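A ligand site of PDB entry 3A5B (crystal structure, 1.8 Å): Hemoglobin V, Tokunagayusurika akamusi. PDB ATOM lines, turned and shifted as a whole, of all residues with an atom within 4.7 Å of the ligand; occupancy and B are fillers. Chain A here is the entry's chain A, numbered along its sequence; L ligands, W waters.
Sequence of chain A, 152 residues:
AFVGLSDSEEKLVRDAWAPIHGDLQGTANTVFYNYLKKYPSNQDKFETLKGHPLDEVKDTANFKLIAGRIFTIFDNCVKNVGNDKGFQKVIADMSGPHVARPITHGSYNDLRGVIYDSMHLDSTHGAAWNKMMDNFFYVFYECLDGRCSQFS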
ATOM      1  N   TYR A  35      -2.429 -28.432   9.205  1.00  0.00           N
ATOM      2  CA  TYR A  35      -1.335 -29.241   8.690  1.00  0.00           C
ATOM      3  C   TYR A  35      -0.893 -30.289   9.702  1.00  0.00           C
ATOM      4  O   TYR A  35      -0.787 -31.478   9.375  1.00  0.00           O
ATOM      5  CB  TYR A  35      -0.152 -28.346   8.316  1.00  0.00           C
ATOM      6  CG  TYR A  35       1.102 -29.087   7.894  1.00  0.00           C
ATOM      7  CD1 TYR A  35       1.113 -29.885   6.754  1.00  0.00           C
ATOM      8  CD2 TYR A  35       2.291 -28.937   8.593  1.00  0.00           C
ATOM      9  CE1 TYR A  35       2.270 -30.517   6.332  1.00  0.00           C
ATOM     10  CE2 TYR A  35       3.452 -29.556   8.182  1.00  0.00           C
ATOM     11  CZ  TYR A  35       3.437 -30.348   7.046  1.00  0.00           C
ATOM     12  OH  TYR A  35       4.595 -30.942   6.619  1.00  0.00           O
ATOM     13  N   ASN A  42       4.542 -34.844  11.258  1.00  0.00           N
ATOM     14  CA  ASN A  42       5.388 -33.671  11.092  1.00  0.00           C
ATOM     15  C   ASN A  42       5.654 -32.888  12.370  1.00  0.00           C
ATOM     16  O   ASN A  42       6.640 -32.150  12.453  1.00  0.00           O
ATOM     17  CB  ASN A  42       4.791 -32.737  10.039  1.00  0.00           C
ATOM     18  CG  ASN A  42       4.794 -33.350   8.675  1.00  0.00           C
ATOM     19  OD1 ASN A  42       5.858 -33.625   8.106  1.00  0.00           O
ATOM     20  ND2 ASN A  42       3.612 -33.586   8.115  1.00  0.00           N
ATOM     21  N   LYS A  45       9.069 -33.002  13.944  1.00  0.00           N
ATOM     22  CA  LYS A  45      10.208 -32.387  13.255  1.00  0.00           C
ATOM     23  C   LYS A  45      10.570 -31.055  13.906  1.00  0.00           C
ATOM     24  O   LYS A  45      11.647 -30.511  13.682  1.00  0.00           O
ATOM     25  CB  LYS A  45       9.885 -32.174  11.778  1.00  0.00           C
ATOM     26  CG  LYS A  45       9.394 -33.425  11.063  1.00  0.00           C
ATOM     27  CD  LYS A  45      10.447 -34.521  11.036  1.00  0.00           C
ATOM     28  CE  LYS A  45       9.887 -35.805  10.447  1.00  0.00           C
ATOM     29  NZ  LYS A  45      10.940 -36.832  10.218  1.00  0.00           N
ATOM     30  N   PHE A  46       9.650 -30.518  14.714  1.00  0.00           N
ATOM     31  CA  PHE A  46       9.873 -29.262  15.410  1.00  0.00           C
ATOM     32  C   PHE A  46      10.163 -29.540  16.881  1.00  0.00           C
ATOM     33  O   PHE A  46       9.240 -29.784  17.665  1.00  0.00           O
ATOM     34  CB  PHE A  46       8.631 -28.366  15.284  1.00  0.00           C
ATOM     35  CG  PHE A  46       8.234 -28.080  13.868  1.00  0.00           C
ATOM     36  CD1 PHE A  46       7.294 -28.865  13.231  1.00  0.00           C
ATOM     37  CD2 PHE A  46       8.800 -27.027  13.175  1.00  0.00           C
ATOM     38  CE1 PHE A  46       6.929 -28.610  11.929  1.00  0.00           C
ATOM     39  CE2 PHE A  46       8.437 -26.757  11.864  1.00  0.00           C
ATOM     40  CZ  PHE A  46       7.496 -27.558  11.246  1.00  0.00           C
ATOM     41  N   ILE A  66       6.574 -20.419  14.373  1.00  0.00           N
ATOM     42  CA  ILE A  66       6.809 -21.345  13.267  1.00  0.00           C
ATOM     43  C   ILE A  66       5.832 -21.121  12.124  1.00  0.00           C
ATOM     44  O   ILE A  66       6.220 -21.048  10.968  1.00  0.00           O
ATOM     45  CB  ILE A  66       6.681 -22.812  13.729  1.00  0.00           C
ATOM     46  CG1 ILE A  66       7.780 -23.136  14.740  1.00  0.00           C
ATOM     47  CG2 ILE A  66       6.765 -23.741  12.519  1.00  0.00           C
ATOM     48  CD1 ILE A  66       7.584 -24.453  15.458  1.00  0.00           C
ATOM     49  N   ARG A  69       6.655 -17.770  10.313  1.00  0.00           N
ATOM     50  CA  ARG A  69       7.865 -17.686   9.509  1.00  0.00           C
ATOM     51  C   ARG A  69       7.662 -18.382   8.157  1.00  0.00           C
ATOM     52  O   ARG A  69       8.196 -17.932   7.146  1.00  0.00           O
ATOM     53  CB  ARG A  69       9.061 -18.292  10.249  1.00  0.00           C
ATOM     54  CG  ARG A  69       9.063 -19.804  10.310  1.00  0.00           C
ATOM     55  CD  ARG A  69      10.236 -20.305  11.151  1.00  0.00           C
ATOM     56  NE  ARG A  69      10.146 -21.748  11.398  1.00  0.00           N
ATOM     57  CZ  ARG A  69      10.690 -22.368  12.437  1.00  0.00           C
ATOM     58  NH1 ARG A  69      11.389 -21.674  13.332  1.00  0.00           N
ATOM     59  NH2 ARG A  69      10.540 -23.670  12.581  1.00  0.00           N
ATOM     60  N   ILE A  70       6.881 -19.455   8.148  1.00  0.00           N
ATOM     61  CA  ILE A  70       6.520 -20.110   6.892  1.00  0.00           C
ATOM     62  C   ILE A  70       5.758 -19.142   5.997  1.00  0.00           C
ATOM     63  O   ILE A  70       6.084 -18.982   4.821  1.00  0.00           O
ATOM     64  CB  ILE A  70       5.625 -21.354   7.145  1.00  0.00           C
ATOM     65  CG1 ILE A  70       6.414 -22.440   7.855  1.00  0.00           C
ATOM     66  CG2 ILE A  70       5.080 -21.875   5.820  1.00  0.00           C
ATOM     67  CD1 ILE A  70       5.552 -23.610   8.330  1.00  0.00           C
ATOM     68  N   ILE A  73       7.812 -16.195   4.494  1.00  0.00           N
ATOM     69  CA  ILE A  73       8.567 -16.585   3.301  1.00  0.00           C
ATOM     70  C   ILE A  73       7.695 -16.548   2.054  1.00  0.00           C
ATOM     71  O   ILE A  73       8.075 -15.950   1.044  1.00  0.00           O
ATOM     72  CB  ILE A  73       9.175 -17.984   3.441  1.00  0.00           C
ATOM     73  CG1 ILE A  73      10.276 -17.965   4.496  1.00  0.00           C
ATOM     74  CG2 ILE A  73       9.738 -18.447   2.096  1.00  0.00           C
ATOM     75  CD1 ILE A  73      11.430 -17.037   4.162  1.00  0.00           C
ATOM     76  N   PHE A  74       6.527 -17.184   2.100  1.00  0.00           N
ATOM     77  CA  PHE A  74       5.643 -17.162   0.944  1.00  0.00           C
ATOM     78  C   PHE A  74       5.172 -15.751   0.626  1.00  0.00           C
ATOM     79  O   PHE A  74       5.044 -15.380  -0.543  1.00  0.00           O
ATOM     80  CB  PHE A  74       4.436 -18.085   1.174  1.00  0.00           C
ATOM     81  CG  PHE A  74       4.771 -19.543   1.052  1.00  0.00           C
ATOM     82  CD1 PHE A  74       5.343 -20.032  -0.105  1.00  0.00           C
ATOM     83  CD2 PHE A  74       4.526 -20.414   2.103  1.00  0.00           C
ATOM     84  CE1 PHE A  74       5.690 -21.370  -0.209  1.00  0.00           C
ATOM     85  CE2 PHE A  74       4.859 -21.748   2.001  1.00  0.00           C
ATOM     86  CZ  PHE A  74       5.440 -22.233   0.845  1.00  0.00           C
ATOM     87  N   MET A  94      16.250 -19.378   2.915  1.00  0.00           N
ATOM     88  CA  MET A  94      15.523 -20.156   3.906  1.00  0.00           C
ATOM     89  C   MET A  94      15.769 -21.658   3.808  1.00  0.00           C
ATOM     90  O   MET A  94      15.370 -22.412   4.683  1.00  0.00           O
ATOM     91  CB  MET A  94      14.012 -19.855   3.819  1.00  0.00           C
ATOM     92  CG  MET A  94      13.392 -20.044   2.444  1.00  0.00           C
ATOM     93  SD  MET A  94      13.218 -21.780   1.920  1.00  0.00           S
ATOM     94  CE  MET A  94      12.092 -22.416   3.094  1.00  0.00           C
ATOM     95  N   PRO A  97      18.264 -24.491   6.798  1.00  0.00           N
ATOM     96  CA  PRO A  97      17.807 -25.291   7.937  1.00  0.00           C
ATOM     97  C   PRO A  97      17.090 -26.576   7.529  1.00  0.00           C
ATOM     98  O   PRO A  97      17.006 -27.520   8.325  1.00  0.00           O
ATOM     99  CB  PRO A  97      16.897 -24.329   8.700  1.00  0.00           C
ATOM    100  CG  PRO A  97      17.402 -22.974   8.328  1.00  0.00           C
ATOM    101  CD  PRO A  97      17.803 -23.097   6.884  1.00  0.00           C
ATOM    102  N   HIS A  98      16.603 -26.646   6.322  1.00  0.00           N
ATOM    103  CA  HIS A  98      15.863 -27.775   5.789  1.00  0.00           C
ATOM    104  C   HIS A  98      16.787 -28.797   5.117  1.00  0.00           C
ATOM    105  O   HIS A  98      16.509 -29.986   5.070  1.00  0.00           O
ATOM    106  CB  HIS A  98      14.841 -27.285   4.756  1.00  0.00           C
ATOM    107  CG  HIS A  98      13.870 -26.306   5.345  1.00  0.00           C
ATOM    108  ND1 HIS A  98      14.106 -24.948   5.271  1.00  0.00           N
ATOM    109  CD2 HIS A  98      12.738 -26.489   6.062  1.00  0.00           C
ATOM    110  CE1 HIS A  98      13.115 -24.333   5.967  1.00  0.00           C
ATOM    111  NE2 HIS A  98      12.275 -25.258   6.448  1.00  0.00           N
ATOM    112  N   ARG A 101      17.827 -31.581   7.726  1.00  0.00           N
ATOM    113  CA  ARG A 101      16.877 -32.300   8.570  1.00  0.00           C
ATOM    114  C   ARG A 101      16.105 -33.402   7.841  1.00  0.00           C
ATOM    115  O   ARG A 101      15.979 -33.380   6.615  1.00  0.00           O
ATOM    116  CB  ARG A 101      15.909 -31.303   9.192  1.00  0.00           C
ATOM    117  CG  ARG A 101      16.600 -30.331  10.134  1.00  0.00           C
ATOM    118  CD  ARG A 101      15.596 -29.507  10.916  1.00  0.00           C
ATOM    119  NE  ARG A 101      16.173 -28.968  12.138  1.00  0.00           N
ATOM    120  CZ  ARG A 101      17.011 -27.931  12.185  1.00  0.00           C
ATOM    121  NH1 ARG A 101      17.364 -27.333  11.057  1.00  0.00           N
ATOM    122  NH2 ARG A 101      17.488 -27.503  13.340  1.00  0.00           N
ATOM    123  N   ILE A 103      13.303 -34.400   6.657  1.00  0.00           N
ATOM    124  CA  ILE A 103      11.987 -33.995   6.186  1.00  0.00           C
ATOM    125  C   ILE A 103      11.800 -34.401   4.735  1.00  0.00           C
ATOM    126  O   ILE A 103      12.623 -34.067   3.875  1.00  0.00           O
ATOM    127  CB  ILE A 103      11.797 -32.467   6.312  1.00  0.00           C
ATOM    128  CG1 ILE A 103      12.092 -32.030   7.744  1.00  0.00           C
ATOM    129  CG2 ILE A 103      10.374 -32.093   5.919  1.00  0.00           C
ATOM    130  CD1 ILE A 103      12.411 -30.546   7.884  1.00  0.00           C
ATOM    131  N   SER A 107       6.270 -34.339   3.077  1.00  0.00           N
ATOM    132  CA  SER A 107       5.933 -33.359   4.102  1.00  0.00           C
ATOM    133  C   SER A 107       5.727 -31.959   3.515  1.00  0.00           C
ATOM    134  O   SER A 107       4.775 -31.265   3.863  1.00  0.00           O
ATOM    135  CB  SER A 107       7.008 -33.314   5.184  1.00  0.00           C
ATOM    136  OG  SER A 107       6.996 -34.486   5.976  1.00  0.00           O
ATOM    137  N   TYR A 108       6.632 -31.548   2.628  1.00  0.00           N
ATOM    138  CA  TYR A 108       6.532 -30.233   2.005  1.00  0.00           C
ATOM    139  C   TYR A 108       5.311 -30.155   1.102  1.00  0.00           C
ATOM    140  O   TYR A 108       4.602 -29.158   1.082  1.00  0.00           O
ATOM    141  CB  TYR A 108       7.789 -29.931   1.180  1.00  0.00           C
ATOM    142  CG  TYR A 108       9.052 -29.885   2.006  1.00  0.00           C
ATOM    143  CD1 TYR A 108       9.201 -28.969   3.034  1.00  0.00           C
ATOM    144  CD2 TYR A 108      10.095 -30.773   1.759  1.00  0.00           C
ATOM    145  CE1 TYR A 108      10.350 -28.928   3.801  1.00  0.00           C
ATOM    146  CE2 TYR A 108      11.248 -30.739   2.515  1.00  0.00           C
ATOM    147  CZ  TYR A 108      11.374 -29.823   3.535  1.00  0.00           C
ATOM    148  OH  TYR A 108      12.519 -29.795   4.301  1.00  0.00           O
ATOM    149  N   LEU A 111       2.113 -29.853   3.041  1.00  0.00           N
ATOM    150  CA  LEU A 111       1.936 -28.474   3.488  1.00  0.00           C
ATOM    151  C   LEU A 111       1.424 -27.592   2.355  1.00  0.00           C
ATOM    152  O   LEU A 111       0.501 -26.795   2.532  1.00  0.00           O
ATOM    153  CB  LEU A 111       3.265 -27.913   4.012  1.00  0.00           C
ATOM    154  CG  LEU A 111       3.239 -26.438   4.416  1.00  0.00           C
ATOM    155  CD1 LEU A 111       2.203 -26.207   5.505  1.00  0.00           C
ATOM    156  CD2 LEU A 111       4.618 -26.026   4.900  1.00  0.00           C
ATOM    157  N   PHE A 136       8.592 -22.239  -6.803  1.00  0.00           N
ATOM    158  CA  PHE A 136       9.109 -22.234  -5.446  1.00  0.00           C
ATOM    159  C   PHE A 136       9.795 -23.558  -5.129  1.00  0.00           C
ATOM    160  O   PHE A 136      10.902 -23.577  -4.611  1.00  0.00           O
ATOM    161  CB  PHE A 136       7.980 -22.004  -4.428  1.00  0.00           C
ATOM    162  CG  PHE A 136       8.415 -22.133  -2.991  1.00  0.00           C
ATOM    163  CD1 PHE A 136       8.798 -21.016  -2.265  1.00  0.00           C
ATOM    164  CD2 PHE A 136       8.452 -23.379  -2.371  1.00  0.00           C
ATOM    165  CE1 PHE A 136       9.209 -21.130  -0.956  1.00  0.00           C
ATOM    166  CE2 PHE A 136       8.864 -23.494  -1.051  1.00  0.00           C
ATOM    167  CZ  PHE A 136       9.245 -22.374  -0.345  1.00  0.00           C
ATOM    168  N   PHE A 137       9.127 -24.661  -5.442  1.00  0.00           N
ATOM    169  CA  PHE A 137       9.651 -25.963  -5.061  1.00  0.00           C
ATOM    170  C   PHE A 137      10.779 -26.446  -5.947  1.00  0.00           C
ATOM    171  O   PHE A 137      11.632 -27.212  -5.509  1.00  0.00           O
ATOM    172  CB  PHE A 137       8.508 -26.985  -5.009  1.00  0.00           C
ATOM    173  CG  PHE A 137       7.743 -26.937  -3.727  1.00  0.00           C
ATOM    174  CD1 PHE A 137       8.256 -27.519  -2.576  1.00  0.00           C
ATOM    175  CD2 PHE A 137       6.533 -26.269  -3.649  1.00  0.00           C
ATOM    176  CE1 PHE A 137       7.588 -27.423  -1.370  1.00  0.00           C
ATOM    177  CE2 PHE A 137       5.859 -26.163  -2.450  1.00  0.00           C
ATOM    178  CZ  PHE A 137       6.389 -26.733  -1.310  1.00  0.00           C
ATOM    179  N   PHE A 140      13.549 -24.641  -4.221  1.00  0.00           N
ATOM    180  CA  PHE A 140      13.726 -25.209  -2.885  1.00  0.00           C
ATOM    181  C   PHE A 140      14.400 -26.574  -2.981  1.00  0.00           C
ATOM    182  O   PHE A 140      15.376 -26.838  -2.283  1.00  0.00           O
ATOM    183  CB  PHE A 140      12.366 -25.338  -2.203  1.00  0.00           C
ATOM    184  CG  PHE A 140      12.447 -25.796  -0.767  1.00  0.00           C
ATOM    185  CD1 PHE A 140      13.211 -25.093   0.152  1.00  0.00           C
ATOM    186  CD2 PHE A 140      11.720 -26.902  -0.339  1.00  0.00           C
ATOM    187  CE1 PHE A 140      13.250 -25.483   1.492  1.00  0.00           C
ATOM    188  CE2 PHE A 140      11.758 -27.290   0.991  1.00  0.00           C
ATOM    189  CZ  PHE A 140      12.514 -26.593   1.911  1.00  0.00           C
HETATM  190  C1  LIG L   1      13.083 -23.468   9.894  1.00  0.00           C
HETATM  191  C2  LIG L   1      10.379 -21.629   6.280  1.00  0.00           C
HETATM  192  C3  LIG L   1       8.560 -26.157   5.593  1.00  0.00           C
HETATM  193  C4  LIG L   1      10.793 -27.801   9.550  1.00  0.00           C
HETATM  194  C5  LIG L   1      12.537 -22.595   8.978  1.00  0.00           C
HETATM  195  C6  LIG L   1      12.903 -21.186   8.846  1.00  0.00           C
HETATM  196  C7  LIG L   1      12.107 -20.648   7.854  1.00  0.00           C
HETATM  197  C8  LIG L   1      11.224 -21.723   7.398  1.00  0.00           C
HETATM  198  C9  LIG L   1      12.023 -19.170   7.429  1.00  0.00           C
HETATM  199  C10 LIG L   1      13.981 -20.474   9.679  1.00  0.00           C
HETATM  200  C11 LIG L   1      15.275 -20.091   8.954  1.00  0.00           C
HETATM  201  C12 LIG L   1      16.261 -19.355   9.863  1.00  0.00           C
HETATM  202  O1  LIG L   1      16.342 -19.743  11.045  1.00  0.00           O
HETATM  203  O2  LIG L   1      16.922 -18.440   9.341  1.00  0.00           O
HETATM  204  C13 LIG L   1       9.709 -22.718   5.745  1.00  0.00           C
HETATM  205  C14 LIG L   1       8.834 -22.651   4.616  1.00  0.00           C
HETATM  206  C15 LIG L   1       8.280 -23.905   4.480  1.00  0.00           C
HETATM  207  C16 LIG L   1       8.873 -24.776   5.452  1.00  0.00           C
HETATM  208  C17 LIG L   1       8.477 -21.378   3.854  1.00  0.00           C
HETATM  209  C18 LIG L   1       7.525 -24.250   3.351  1.00  0.00           C
HETATM  210  C19 LIG L   1       7.788 -25.301   2.345  1.00  0.00           C
HETATM  211  C20 LIG L   1       8.919 -26.935   6.659  1.00  0.00           C
HETATM  212  C21 LIG L   1       8.350 -28.247   6.892  1.00  0.00           C
HETATM  213  C22 LIG L   1       8.928 -28.679   8.059  1.00  0.00           C
HETATM  214  C23 LIG L   1       9.942 -27.694   8.465  1.00  0.00           C
HETATM  215  C24 LIG L   1       7.264 -28.926   6.045  1.00  0.00           C
HETATM  216  C25 LIG L   1       8.690 -29.985   8.723  1.00  0.00           C
HETATM  217  C26 LIG L   1      11.638 -26.761   9.963  1.00  0.00           C
HETATM  218  C27 LIG L   1      12.501 -26.845  11.132  1.00  0.00           C
HETATM  219  C28 LIG L   1      13.332 -25.655  11.215  1.00  0.00           C
HETATM  220  C29 LIG L   1      12.749 -24.829  10.102  1.00  0.00           C
HETATM  221  C30 LIG L   1      12.606 -28.033  12.081  1.00  0.00           C
HETATM  222  C31 LIG L   1      14.558 -25.129  12.307  1.00  0.00           C
HETATM  223  C32 LIG L   1      13.817 -24.691  13.322  1.00  0.00           C
HETATM  224  C33 LIG L   1      13.149 -25.449  14.371  1.00  0.00           C
HETATM  225  O3  LIG L   1      14.067 -26.134  15.079  1.00  0.00           O
HETATM  226  O4  LIG L   1      11.962 -25.398  14.591  1.00  0.00           O
HETATM  227  N1  LIG L   1      11.564 -22.852   8.053  1.00  0.00           N
HETATM  228  N2  LIG L   1       9.674 -24.005   6.215  1.00  0.00           N
HETATM  229  N3  LIG L   1       9.814 -26.603   7.626  1.00  0.00           N
HETATM  230  N4  LIG L   1      11.772 -25.508   9.425  1.00  0.00           N
HETATM  231 FE1  LIG L   1      10.711 -24.716   7.844  1.00  0.00          FE
HETATM  232  O   HOH W   1      13.296 -28.888  15.277  1.00  0.00           O
HETATM  233  O   HOH W   2      14.205 -25.937  17.991  1.00  0.00           O
HETATM  234  O   HOH W   3      10.354 -16.134   7.801  1.00  0.00           O
HETATM  235  O   HOH W   4      17.170 -22.802  11.922  1.00  0.00           O
HETATM  236  O   HOH W   5      11.168 -26.426  16.764  1.00  0.00           O
HETATM  237  O   HOH W   6      11.240 -22.883  16.409  1.00  0.00           O
HETATM  238  O   HOH W   7      13.471 -16.062   7.411  1.00  0.00           O
HETATM  239  O   HOH W   8       9.048 -24.086   9.530  1.00  0.00           O
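ND2 of Asn 42 sits close to OH of Tyr 35. NH1 of Arg 101 sits at hydrogen-bond distance from O of Pro 97 (2.8 Å). O of Met 94 is in hydrogen-bond range of ND1 of His 98 (2.9 Å). O of Ser 107 sits at hydrogen-bond distance from OH of Tyr 35 (2.8 Å).
NE2 of His 98 is bound to FE1 of the ligand. The guanidinium group of Arg 69 is in salt-bridge range of an oxygen (O4) of the ligand.
Water W1 lies within hydrogen-bond range of O of Lys 45 (2.8 Å) and O3 of the ligand (2.9 Å). Water W6 lies within hydrogen-bond range of an oxygen (O4) of the ligand and the guanidinium group of Arg 69.
Residues that only touch the ligand: Lys 45 (3.1 Å), Tyr 35 (3.4 Å), Phe 46 (3.5 Å), Ile 73 (3.5 Å), Ile 70 (3.5 Å), Arg 101 (3.5 Å), Met 94 (3.6 Å), Tyr 108 (3.6 Å), Ile 103 (3.6 Å), Pro 97 (3.6 Å), Leu 111 (3.7 Å), Phe 74 (3.8 Å) and Phe 136 (3.99 Å). Hydrophobic or aromatic side chains that line the ligand: Phe 46, Ile 70, Ile 73, Phe 74, Met 94, Pro 97, His 98, Ile 103, Tyr 108, Leu 111 and Phe 136. Within 4 Å of the ligand: Tyr 35, Lys 45, Phe 46, Arg 69, Ile 70, Ile 73, Phe 74, Met 94, Pro 97, His 98, Arg 101, Ile 103, Tyr 108, Leu 111 and Phe 136. The nearest printed residue that does not touch the ligand is Ser 107 (4.1 Å).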
